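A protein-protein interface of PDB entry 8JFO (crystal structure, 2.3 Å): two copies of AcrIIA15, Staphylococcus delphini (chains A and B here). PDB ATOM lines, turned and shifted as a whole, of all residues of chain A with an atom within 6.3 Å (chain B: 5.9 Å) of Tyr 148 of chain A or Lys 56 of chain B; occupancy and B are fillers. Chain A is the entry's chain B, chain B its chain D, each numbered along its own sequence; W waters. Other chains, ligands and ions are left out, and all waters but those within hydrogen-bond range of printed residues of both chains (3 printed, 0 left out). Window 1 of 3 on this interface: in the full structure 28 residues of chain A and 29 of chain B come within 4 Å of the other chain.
Lys 56 of chain B touches one residue of chain A. Of the printed residues of chain B, Glu 146 of chain A touches Thr 5 and Arg 8. Printed residues of chain B within 4 Å of Lys 113 of chain A: Arg 8 (3.5 Å) and Glu 59 (3.2 Å). Of the printed residues of chain A, Thr 5 of chain B touches Glu 146 and Tyr 148. Of the printed residues of chain A, Glu 59 of chain B touches Lys 113. Of the printed residues of chain A, Arg 8 of chain B touches Lys 113, Glu 146 and Tyr 148. Leu 51 of chain B touches none of the printed residues of chain A. Tyr 54 of chain B touches none of the printed residues of chain A. The nearest printed residue of chain A that does not touch Lys 56 of chain B is Glu 152 of chain A (6.4 Å). The nearest printed residue of chain B that does not touch Lys 113 of chain A is Thr 5 of chain B (5.1 Å).
The backbone carbonyl oxygen (O) of Lys 113 of chain A lies close to the side-chain carboxylate (OE2) of Glu 59 of chain B (3.2 Å). The side-chain amino group (NZ) of Lys 113 of chain A sits close to the guanidinium group (NH2) of Arg 8 of chain B (3.5 Å). The side-chain carboxylate (OE2) of Glu 146 of chain A is in salt-bridge range of the guanidinium group (NH1) of Arg 8 of chain B, at 3.8 Å.
Water W3 bridges OH of Tyr 148 of chain A and OE1 of Glu 59 of chain B. Water W2 bridges the backbone carbonyl oxygen (O) of Glu 59 of chain B (2.7 Å) and the side-chain amide nitrogen (NE2) of Gln 109 of chain A (2.8 Å). Water W1 lies within hydrogen-bond range of the side-chain carboxylate of Glu 59 of chain B (2.8 Å) and the backbone carbonyl oxygen of Lys 113 of chain A (2.8 Å).
Of the 12 printed residues of chain B, 4 touch a printed residue of chain A. Among the printed residues, 7 pairs touch across the chains.
Among the printed residues, merely in contact across the chains: Glu 146 of chain A with Thr 5 of chain B (3.8 Å), Tyr 148 of chain A with Arg 8 of chain B (3.8 Å), Tyr 148 of chain A with Thr 5 of chain B (3.9 Å) and Tyr 148 of chain A with Lys 56 of chain B (3.9 Å).
The guanidinium group (NE) of Arg 8 of chain B is in salt-bridge range of the side-chain carboxylate (OE2) of Glu 59 of chain B. The guanidinium group of Arg 8 of chain B lies within hydrogen-bond range of the side-chain hydroxyl of Thr 5 of chain B, at 3.1 Å. The side-chain amino group of Lys 113 of chain A lies within salt-bridge range of the side-chain carboxylate of Asp 149 of chain A. The side-chain carboxylate (OE2) of Glu 53 of chain B is in salt-bridge range of the side-chain amino group (NZ) of Lys 56 of chain B. NZ of Lys 113 of chain A sits at hydrogen-bond distance from OH of Tyr 148 of chain A (3.2 Å). The backbone NH (N) of Glu 146 of chain A lies within hydrogen-bond range of the side-chain carboxylate (OD2) of Asp 149 of chain A (2.8 Å).
No position is printed for both chains. Of the 7 pairs that touch across the chains among the printed residues, none has its exchanged pair printed and touching as well.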
ATOM      1  N   TYR A  85     -27.556  -8.927  15.337  1.00  0.00           N
ATOM      2  CA  TYR A  85     -26.570  -8.695  16.387  1.00  0.00           C
ATOM      3  C   TYR A  85     -25.201  -8.430  15.795  1.00  0.00           C
ATOM      4  O   TYR A  85     -24.447  -7.604  16.321  1.00  0.00           O
ATOM      5  CB  TYR A  85     -26.507  -9.884  17.333  1.00  0.00           C
ATOM      6  CG  TYR A  85     -27.732 -10.007  18.177  1.00  0.00           C
ATOM      7  CD1 TYR A  85     -28.111  -8.982  19.031  1.00  0.00           C
ATOM      8  CD2 TYR A  85     -28.503 -11.151  18.138  1.00  0.00           C
ATOM      9  CE1 TYR A  85     -29.235  -9.093  19.814  1.00  0.00           C
ATOM     10  CE2 TYR A  85     -29.617 -11.275  18.921  1.00  0.00           C
ATOM     11  CZ  TYR A  85     -29.984 -10.244  19.750  1.00  0.00           C
ATOM     12  OH  TYR A  85     -31.105 -10.376  20.531  1.00  0.00           O
ATOM     13  N   GLN A 109     -14.312 -16.048  22.259  1.00  0.00           N
ATOM     14  CA  GLN A 109     -15.596 -16.652  21.931  1.00  0.00           C
ATOM     15  C   GLN A 109     -15.480 -17.599  20.738  1.00  0.00           C
ATOM     16  O   GLN A 109     -16.077 -18.680  20.734  1.00  0.00           O
ATOM     17  CB  GLN A 109     -16.614 -15.561  21.634  1.00  0.00           C
ATOM     18  CG  GLN A 109     -17.995 -16.091  21.349  1.00  0.00           C
ATOM     19  CD  GLN A 109     -18.970 -15.751  22.437  1.00  0.00           C
ATOM     20  OE1 GLN A 109     -18.920 -14.663  23.019  1.00  0.00           O
ATOM     21  NE2 GLN A 109     -19.857 -16.688  22.744  1.00  0.00           N
ATOM     22  N   LYS A 113     -16.248 -21.550  20.799  1.00  0.00           N
ATOM     23  CA  LYS A 113     -17.247 -22.122  19.899  1.00  0.00           C
ATOM     24  C   LYS A 113     -16.680 -23.303  19.128  1.00  0.00           C
ATOM     25  O   LYS A 113     -17.422 -24.218  18.766  1.00  0.00           O
ATOM     26  CB  LYS A 113     -17.759 -21.064  18.925  1.00  0.00           C
ATOM     27  CG  LYS A 113     -19.021 -21.471  18.169  1.00  0.00           C
ATOM     28  CD  LYS A 113     -19.270 -20.588  16.944  1.00  0.00           C
ATOM     29  CE  LYS A 113     -20.615 -20.903  16.294  1.00  0.00           C
ATOM     30  NZ  LYS A 113     -21.744 -20.603  17.214  1.00  0.00           N
ATOM     31  N   GLU A 146     -21.874 -17.431  14.885  1.00  0.00           N
ATOM     32  CA  GLU A 146     -23.242 -17.218  14.431  1.00  0.00           C
ATOM     33  C   GLU A 146     -23.772 -15.919  15.033  1.00  0.00           C
ATOM     34  O   GLU A 146     -23.079 -15.239  15.791  1.00  0.00           O
ATOM     35  CB  GLU A 146     -24.113 -18.416  14.798  1.00  0.00           C
ATOM     36  CG  GLU A 146     -23.869 -19.628  13.898  1.00  0.00           C
ATOM     37  CD  GLU A 146     -24.051 -20.962  14.621  1.00  0.00           C
ATOM     38  OE1 GLU A 146     -24.216 -20.970  15.860  1.00  0.00           O
ATOM     39  OE2 GLU A 146     -24.042 -22.011  13.947  1.00  0.00           O
ATOM     40  N   ASP A 147     -25.008 -15.548  14.682  1.00  0.00           N
ATOM     41  CA  ASP A 147     -25.507 -14.231  15.078  1.00  0.00           C
ATOM     42  C   ASP A 147     -25.639 -14.080  16.595  1.00  0.00           C
ATOM     43  O   ASP A 147     -25.334 -13.014  17.142  1.00  0.00           O
ATOM     44  CB  ASP A 147     -26.840 -13.920  14.400  1.00  0.00           C
ATOM     45  CG  ASP A 147     -27.126 -12.421  14.363  1.00  0.00           C
ATOM     46  OD1 ASP A 147     -26.274 -11.668  13.843  1.00  0.00           O
ATOM     47  OD2 ASP A 147     -28.174 -11.984  14.886  1.00  0.00           O
ATOM     48  N   TYR A 148     -26.125 -15.111  17.291  1.00  0.00           N
ATOM     49  CA  TYR A 148     -26.303 -14.984  18.739  1.00  0.00           C
ATOM     50  C   TYR A 148     -24.965 -14.754  19.438  1.00  0.00           C
ATOM     51  O   TYR A 148     -24.904 -14.137  20.513  1.00  0.00           O
ATOM     52  CB  TYR A 148     -27.032 -16.219  19.296  1.00  0.00           C
ATOM     53  CG  TYR A 148     -26.212 -17.504  19.345  1.00  0.00           C
ATOM     54  CD1 TYR A 148     -25.377 -17.789  20.432  1.00  0.00           C
ATOM     55  CD2 TYR A 148     -26.274 -18.433  18.303  1.00  0.00           C
ATOM     56  CE1 TYR A 148     -24.624 -18.958  20.473  1.00  0.00           C
ATOM     57  CE2 TYR A 148     -25.525 -19.608  18.337  1.00  0.00           C
ATOM     58  CZ  TYR A 148     -24.702 -19.866  19.427  1.00  0.00           C
ATOM     59  OH  TYR A 148     -23.954 -21.030  19.472  1.00  0.00           O
ATOM     60  N   ASP A 149     -23.879 -15.218  18.826  1.00  0.00           N
ATOM     61  CA  ASP A 149     -22.564 -15.016  19.411  1.00  0.00           C
ATOM     62  C   ASP A 149     -22.215 -13.537  19.539  1.00  0.00           C
ATOM     63  O   ASP A 149     -21.497 -13.160  20.470  1.00  0.00           O
ATOM     64  CB  ASP A 149     -21.516 -15.748  18.572  1.00  0.00           C
ATOM     65  CG  ASP A 149     -21.670 -17.257  18.641  1.00  0.00           C
ATOM     66  OD1 ASP A 149     -21.893 -17.750  19.765  1.00  0.00           O
ATOM     67  OD2 ASP A 149     -21.571 -17.946  17.594  1.00  0.00           O
ATOM     68  N   TYR A 150     -22.714 -12.675  18.636  1.00  0.00           N
ATOM     69  CA  TYR A 150     -22.399 -11.245  18.733  1.00  0.00           C
ATOM     70  C   TYR A 150     -23.093 -10.593  19.932  1.00  0.00           C
ATOM     71  O   TYR A 150     -22.490  -9.766  20.659  1.00  0.00           O
ATOM     72  CB  TYR A 150     -22.733 -10.550  17.409  1.00  0.00           C
ATOM     73  CG  TYR A 150     -21.772 -10.983  16.316  1.00  0.00           C
ATOM     74  CD1 TYR A 150     -20.533 -10.380  16.189  1.00  0.00           C
ATOM     75  CD2 TYR A 150     -22.086 -12.020  15.444  1.00  0.00           C
ATOM     76  CE1 TYR A 150     -19.633 -10.785  15.218  1.00  0.00           C
ATOM     77  CE2 TYR A 150     -21.194 -12.428  14.464  1.00  0.00           C
ATOM     78  CZ  TYR A 150     -19.966 -11.806  14.356  1.00  0.00           C
ATOM     79  OH  TYR A 150     -19.057 -12.199  13.393  1.00  0.00           O
ATOM     80  N   ARG A 151     -24.303 -11.049  20.249  1.00  0.00           N
ATOM     81  CA  ARG A 151     -24.948 -10.540  21.487  1.00  0.00           C
ATOM     82  C   ARG A 151     -24.072 -10.960  22.670  1.00  0.00           C
ATOM     83  O   ARG A 151     -23.869 -10.132  23.565  1.00  0.00           O
ATOM     84  CB  ARG A 151     -26.359 -11.111  21.641  1.00  0.00           C
ATOM     85  CG  ARG A 151     -27.137 -10.548  22.821  1.00  0.00           C
ATOM     86  CD  ARG A 151     -28.425 -11.305  23.068  1.00  0.00           C
ATOM     87  NE  ARG A 151     -29.062 -10.900  24.311  1.00  0.00           N
ATOM     88  CZ  ARG A 151     -30.165 -10.166  24.394  1.00  0.00           C
ATOM     89  NH1 ARG A 151     -30.779  -9.766  23.297  1.00  0.00           N
ATOM     90  NH2 ARG A 151     -30.658  -9.851  25.577  1.00  0.00           N
ATOM     91  N   GLU A 152     -23.540 -12.181  22.632  1.00  0.00           N
ATOM     92  CA  GLU A 152     -22.695 -12.726  23.729  1.00  0.00           C
ATOM     93  C   GLU A 152     -21.399 -11.918  23.908  1.00  0.00           C
ATOM     94  O   GLU A 152     -20.951 -11.799  25.050  1.00  0.00           O
ATOM     95  CB  GLU A 152     -22.473 -14.226  23.532  1.00  0.00           C
ATOM     96  CG  GLU A 152     -23.734 -15.043  23.733  1.00  0.00           C
ATOM     97  CD  GLU A 152     -24.275 -15.001  25.150  1.00  0.00           C
ATOM     98  OE1 GLU A 152     -23.522 -15.351  26.079  1.00  0.00           O
ATOM     99  OE2 GLU A 152     -25.443 -14.606  25.322  1.00  0.00           O
ATOM    100  N   LEU A 153     -20.827 -11.393  22.820  1.00  0.00           N
ATOM    101  CA  LEU A 153     -19.580 -10.597  22.919  1.00  0.00           C
ATOM    102  C   LEU A 153     -19.851  -9.413  23.850  1.00  0.00           C
ATOM    103  O   LEU A 153     -18.983  -9.122  24.682  1.00  0.00           O
ATOM    104  CB  LEU A 153     -19.165 -10.123  21.523  1.00  0.00           C
ATOM    105  CG  LEU A 153     -18.774 -11.212  20.529  1.00  0.00           C
ATOM    106  CD1 LEU A 153     -18.335 -10.599  19.212  1.00  0.00           C
ATOM    107  CD2 LEU A 153     -17.671 -12.084  21.096  1.00  0.00           C
ATOM    108  N   THR B   5     -25.320 -26.301  15.870  1.00  0.00           N
ATOM    109  CA  THR B   5     -24.892 -26.476  17.250  1.00  0.00           C
ATOM    110  C   THR B   5     -25.181 -27.888  17.742  1.00  0.00           C
ATOM    111  O   THR B   5     -24.334 -28.514  18.395  1.00  0.00           O
ATOM    112  CB  THR B   5     -25.569 -25.429  18.128  1.00  0.00           C
ATOM    113  OG1 THR B   5     -25.362 -24.137  17.548  1.00  0.00           O
ATOM    114  CG2 THR B   5     -24.986 -25.447  19.519  1.00  0.00           C
ATOM    115  N   ARG B   8     -22.627 -30.183  16.364  1.00  0.00           N
ATOM    116  CA  ARG B   8     -21.349 -30.086  17.118  1.00  0.00           C
ATOM    117  C   ARG B   8     -21.453 -30.942  18.381  1.00  0.00           C
ATOM    118  O   ARG B   8     -20.471 -31.625  18.699  1.00  0.00           O
ATOM    119  CB  ARG B   8     -20.956 -28.632  17.390  1.00  0.00           C
ATOM    120  CG  ARG B   8     -20.568 -27.842  16.150  1.00  0.00           C
ATOM    121  CD  ARG B   8     -19.931 -26.501  16.471  1.00  0.00           C
ATOM    122  NE  ARG B   8     -20.740 -25.630  17.312  1.00  0.00           N
ATOM    123  CZ  ARG B   8     -21.615 -24.737  16.864  1.00  0.00           C
ATOM    124  NH1 ARG B   8     -21.816 -24.591  15.568  1.00  0.00           N
ATOM    125  NH2 ARG B   8     -22.288 -23.991  17.719  1.00  0.00           N
ATOM    126  N   LEU B  51     -30.850 -30.268  23.643  1.00  0.00           N
ATOM    127  CA  LEU B  51     -29.516 -30.509  23.093  1.00  0.00           C
ATOM    128  C   LEU B  51     -28.797 -29.194  22.769  1.00  0.00           C
ATOM    129  O   LEU B  51     -27.594 -29.043  23.036  1.00  0.00           O
ATOM    130  CB  LEU B  51     -29.620 -31.386  21.847  1.00  0.00           C
ATOM    131  CG  LEU B  51     -30.186 -32.796  22.041  1.00  0.00           C
ATOM    132  CD1 LEU B  51     -30.169 -33.558  20.719  1.00  0.00           C
ATOM    133  CD2 LEU B  51     -29.416 -33.561  23.105  1.00  0.00           C
ATOM    134  N   PHE B  52     -29.521 -28.241  22.176  1.00  0.00           N
ATOM    135  CA  PHE B  52     -28.940 -26.962  21.792  1.00  0.00           C
ATOM    136  C   PHE B  52     -28.459 -26.172  23.011  1.00  0.00           C
ATOM    137  O   PHE B  52     -27.347 -25.633  23.006  1.00  0.00           O
ATOM    138  CB  PHE B  52     -29.990 -26.188  21.005  1.00  0.00           C
ATOM    139  CG  PHE B  52     -29.600 -24.783  20.635  1.00  0.00           C
ATOM    140  CD1 PHE B  52     -28.661 -24.546  19.638  1.00  0.00           C
ATOM    141  CD2 PHE B  52     -30.220 -23.701  21.239  1.00  0.00           C
ATOM    142  CE1 PHE B  52     -28.321 -23.256  19.275  1.00  0.00           C
ATOM    143  CE2 PHE B  52     -29.897 -22.411  20.875  1.00  0.00           C
ATOM    144  CZ  PHE B  52     -28.943 -22.184  19.893  1.00  0.00           C
ATOM    145  N   GLU B  53     -29.271 -26.131  24.068  1.00  0.00           N
ATOM    146  CA  GLU B  53     -28.912 -25.362  25.288  1.00  0.00           C
ATOM    147  C   GLU B  53     -27.707 -25.992  25.989  1.00  0.00           C
ATOM    148  O   GLU B  53     -26.857 -25.234  26.475  1.00  0.00           O
ATOM    149  CB  GLU B  53     -30.100 -25.245  26.240  1.00  0.00           C
ATOM    150  CG  GLU B  53     -31.176 -24.296  25.741  1.00  0.00           C
ATOM    151  CD  GLU B  53     -30.745 -22.845  25.607  1.00  0.00           C
ATOM    152  OE1 GLU B  53     -29.953 -22.382  26.449  1.00  0.00           O
ATOM    153  OE2 GLU B  53     -31.199 -22.182  24.656  1.00  0.00           O
ATOM    154  N   TYR B  54     -27.642 -27.322  26.035  1.00  0.00           N
ATOM    155  CA  TYR B  54     -26.465 -27.994  26.638  1.00  0.00           C
ATOM    156  C   TYR B  54     -25.206 -27.685  25.815  1.00  0.00           C
ATOM    157  O   TYR B  54     -24.175 -27.379  26.425  1.00  0.00           O
ATOM    158  CB  TYR B  54     -26.678 -29.497  26.817  1.00  0.00           C
ATOM    159  CG  TYR B  54     -25.466 -30.211  27.358  1.00  0.00           C
ATOM    160  CD1 TYR B  54     -25.108 -30.098  28.690  1.00  0.00           C
ATOM    161  CD2 TYR B  54     -24.662 -30.977  26.534  1.00  0.00           C
ATOM    162  CE1 TYR B  54     -23.989 -30.739  29.193  1.00  0.00           C
ATOM    163  CE2 TYR B  54     -23.539 -31.623  27.020  1.00  0.00           C
ATOM    164  CZ  TYR B  54     -23.202 -31.504  28.354  1.00  0.00           C
ATOM    165  OH  TYR B  54     -22.092 -32.134  28.833  1.00  0.00           O
ATOM    166  N   GLN B  55     -25.289 -27.769  24.487  1.00  0.00           N
ATOM    167  CA  GLN B  55     -24.082 -27.466  23.712  1.00  0.00           C
ATOM    168  C   GLN B  55     -23.671 -26.002  23.857  1.00  0.00           C
ATOM    169  O   GLN B  55     -22.473 -25.689  23.872  1.00  0.00           O
ATOM    170  CB  GLN B  55     -24.258 -27.819  22.236  1.00  0.00           C
ATOM    171  CG  GLN B  55     -22.997 -27.568  21.381  1.00  0.00           C
ATOM    172  CD  GLN B  55     -21.825 -28.458  21.730  1.00  0.00           C
ATOM    173  OE1 GLN B  55     -21.964 -29.440  22.452  1.00  0.00           O
ATOM    174  NE2 GLN B  55     -20.654 -28.116  21.212  1.00  0.00           N
ATOM    175  N   LYS B  56     -24.640 -25.095  23.953  1.00  0.00           N
ATOM    176  CA  LYS B  56     -24.323 -23.656  24.148  1.00  0.00           C
ATOM    177  C   LYS B  56     -23.569 -23.472  25.468  1.00  0.00           C
ATOM    178  O   LYS B  56     -22.605 -22.701  25.484  1.00  0.00           O
ATOM    179  CB  LYS B  56     -25.589 -22.799  24.101  1.00  0.00           C
ATOM    180  CG  LYS B  56     -25.782 -22.005  22.818  1.00  0.00           C
ATOM    181  CD  LYS B  56     -27.111 -21.290  22.769  1.00  0.00           C
ATOM    182  CE  LYS B  56     -27.443 -20.554  24.047  1.00  0.00           C
ATOM    183  NZ  LYS B  56     -28.857 -20.113  24.071  1.00  0.00           N
ATOM    184  N   GLU B  57     -23.998 -24.163  26.522  1.00  0.00           N
ATOM    185  CA  GLU B  57     -23.317 -24.094  27.839  1.00  0.00           C
ATOM    186  C   GLU B  57     -21.895 -24.642  27.699  1.00  0.00           C
ATOM    187  O   GLU B  57     -20.980 -24.080  28.317  1.00  0.00           O
ATOM    188  CB  GLU B  57     -24.139 -24.861  28.875  1.00  0.00           C
ATOM    189  CG  GLU B  57     -23.428 -25.070  30.197  1.00  0.00           C
ATOM    190  CD  GLU B  57     -24.121 -26.047  31.130  1.00  0.00           C
ATOM    191  OE1 GLU B  57     -25.198 -26.552  30.760  1.00  0.00           O
ATOM    192  OE2 GLU B  57     -23.579 -26.304  32.223  1.00  0.00           O
ATOM    193  N   MET B  58     -21.729 -25.702  26.913  1.00  0.00           N
ATOM    194  CA  MET B  58     -20.391 -26.304  26.707  1.00  0.00           C
ATOM    195  C   MET B  58     -19.484 -25.302  25.986  1.00  0.00           C
ATOM    196  O   MET B  58     -18.262 -25.415  26.140  1.00  0.00           O
ATOM    197  CB  MET B  58     -20.483 -27.612  25.917  1.00  0.00           C
ATOM    198  CG  MET B  58     -21.120 -28.746  26.694  1.00  0.00           C
ATOM    199  SD  MET B  58     -20.213 -29.160  28.204  1.00  0.00           S
ATOM    200  CE  MET B  58     -21.224 -28.357  29.448  1.00  0.00           C
ATOM    201  N   GLU B  59     -20.065 -24.362  25.242  1.00  0.00           N
ATOM    202  CA  GLU B  59     -19.231 -23.407  24.465  1.00  0.00           C
ATOM    203  C   GLU B  59     -19.308 -22.020  25.105  1.00  0.00           C
ATOM    204  O   GLU B  59     -18.825 -21.064  24.490  1.00  0.00           O
ATOM    205  CB  GLU B  59     -19.715 -23.349  23.016  1.00  0.00           C
ATOM    206  CG  GLU B  59     -19.522 -24.640  22.248  1.00  0.00           C
ATOM    207  CD  GLU B  59     -20.389 -24.758  21.007  1.00  0.00           C
ATOM    208  OE1 GLU B  59     -21.427 -24.076  20.949  1.00  0.00           O
ATOM    209  OE2 GLU B  59     -20.036 -25.542  20.111  1.00  0.00           O
ATOM    210  N   LYS B  60     -19.886 -21.928  26.298  1.00  0.00           N
ATOM    211  CA  LYS B  60     -20.076 -20.609  26.945  1.00  0.00           C
ATOM    212  C   LYS B  60     -18.744 -20.058  27.446  1.00  0.00           C
ATOM    213  O   LYS B  60     -17.955 -20.834  28.013  1.00  0.00           O
ATOM    214  CB  LYS B  60     -21.088 -20.701  28.088  1.00  0.00           C
ATOM    215  CG  LYS B  60     -21.646 -19.374  28.583  1.00  0.00           C
ATOM    216  CD  LYS B  60     -22.705 -19.541  29.651  1.00  0.00           C
ATOM    217  CE  LYS B  60     -23.300 -18.231  30.115  1.00  0.00           C
ATOM    218  NZ  LYS B  60     -22.278 -17.350  30.729  1.00  0.00           N
HETATM  219  O   HOH W   1     -17.515 -26.838  19.881  1.00  0.00           O
HETATM  220  O   HOH W   2     -18.554 -19.202  22.566  1.00  0.00           O
HETATM  221  O   HOH W   3     -21.813 -21.445  20.651  1.00  0.00           O
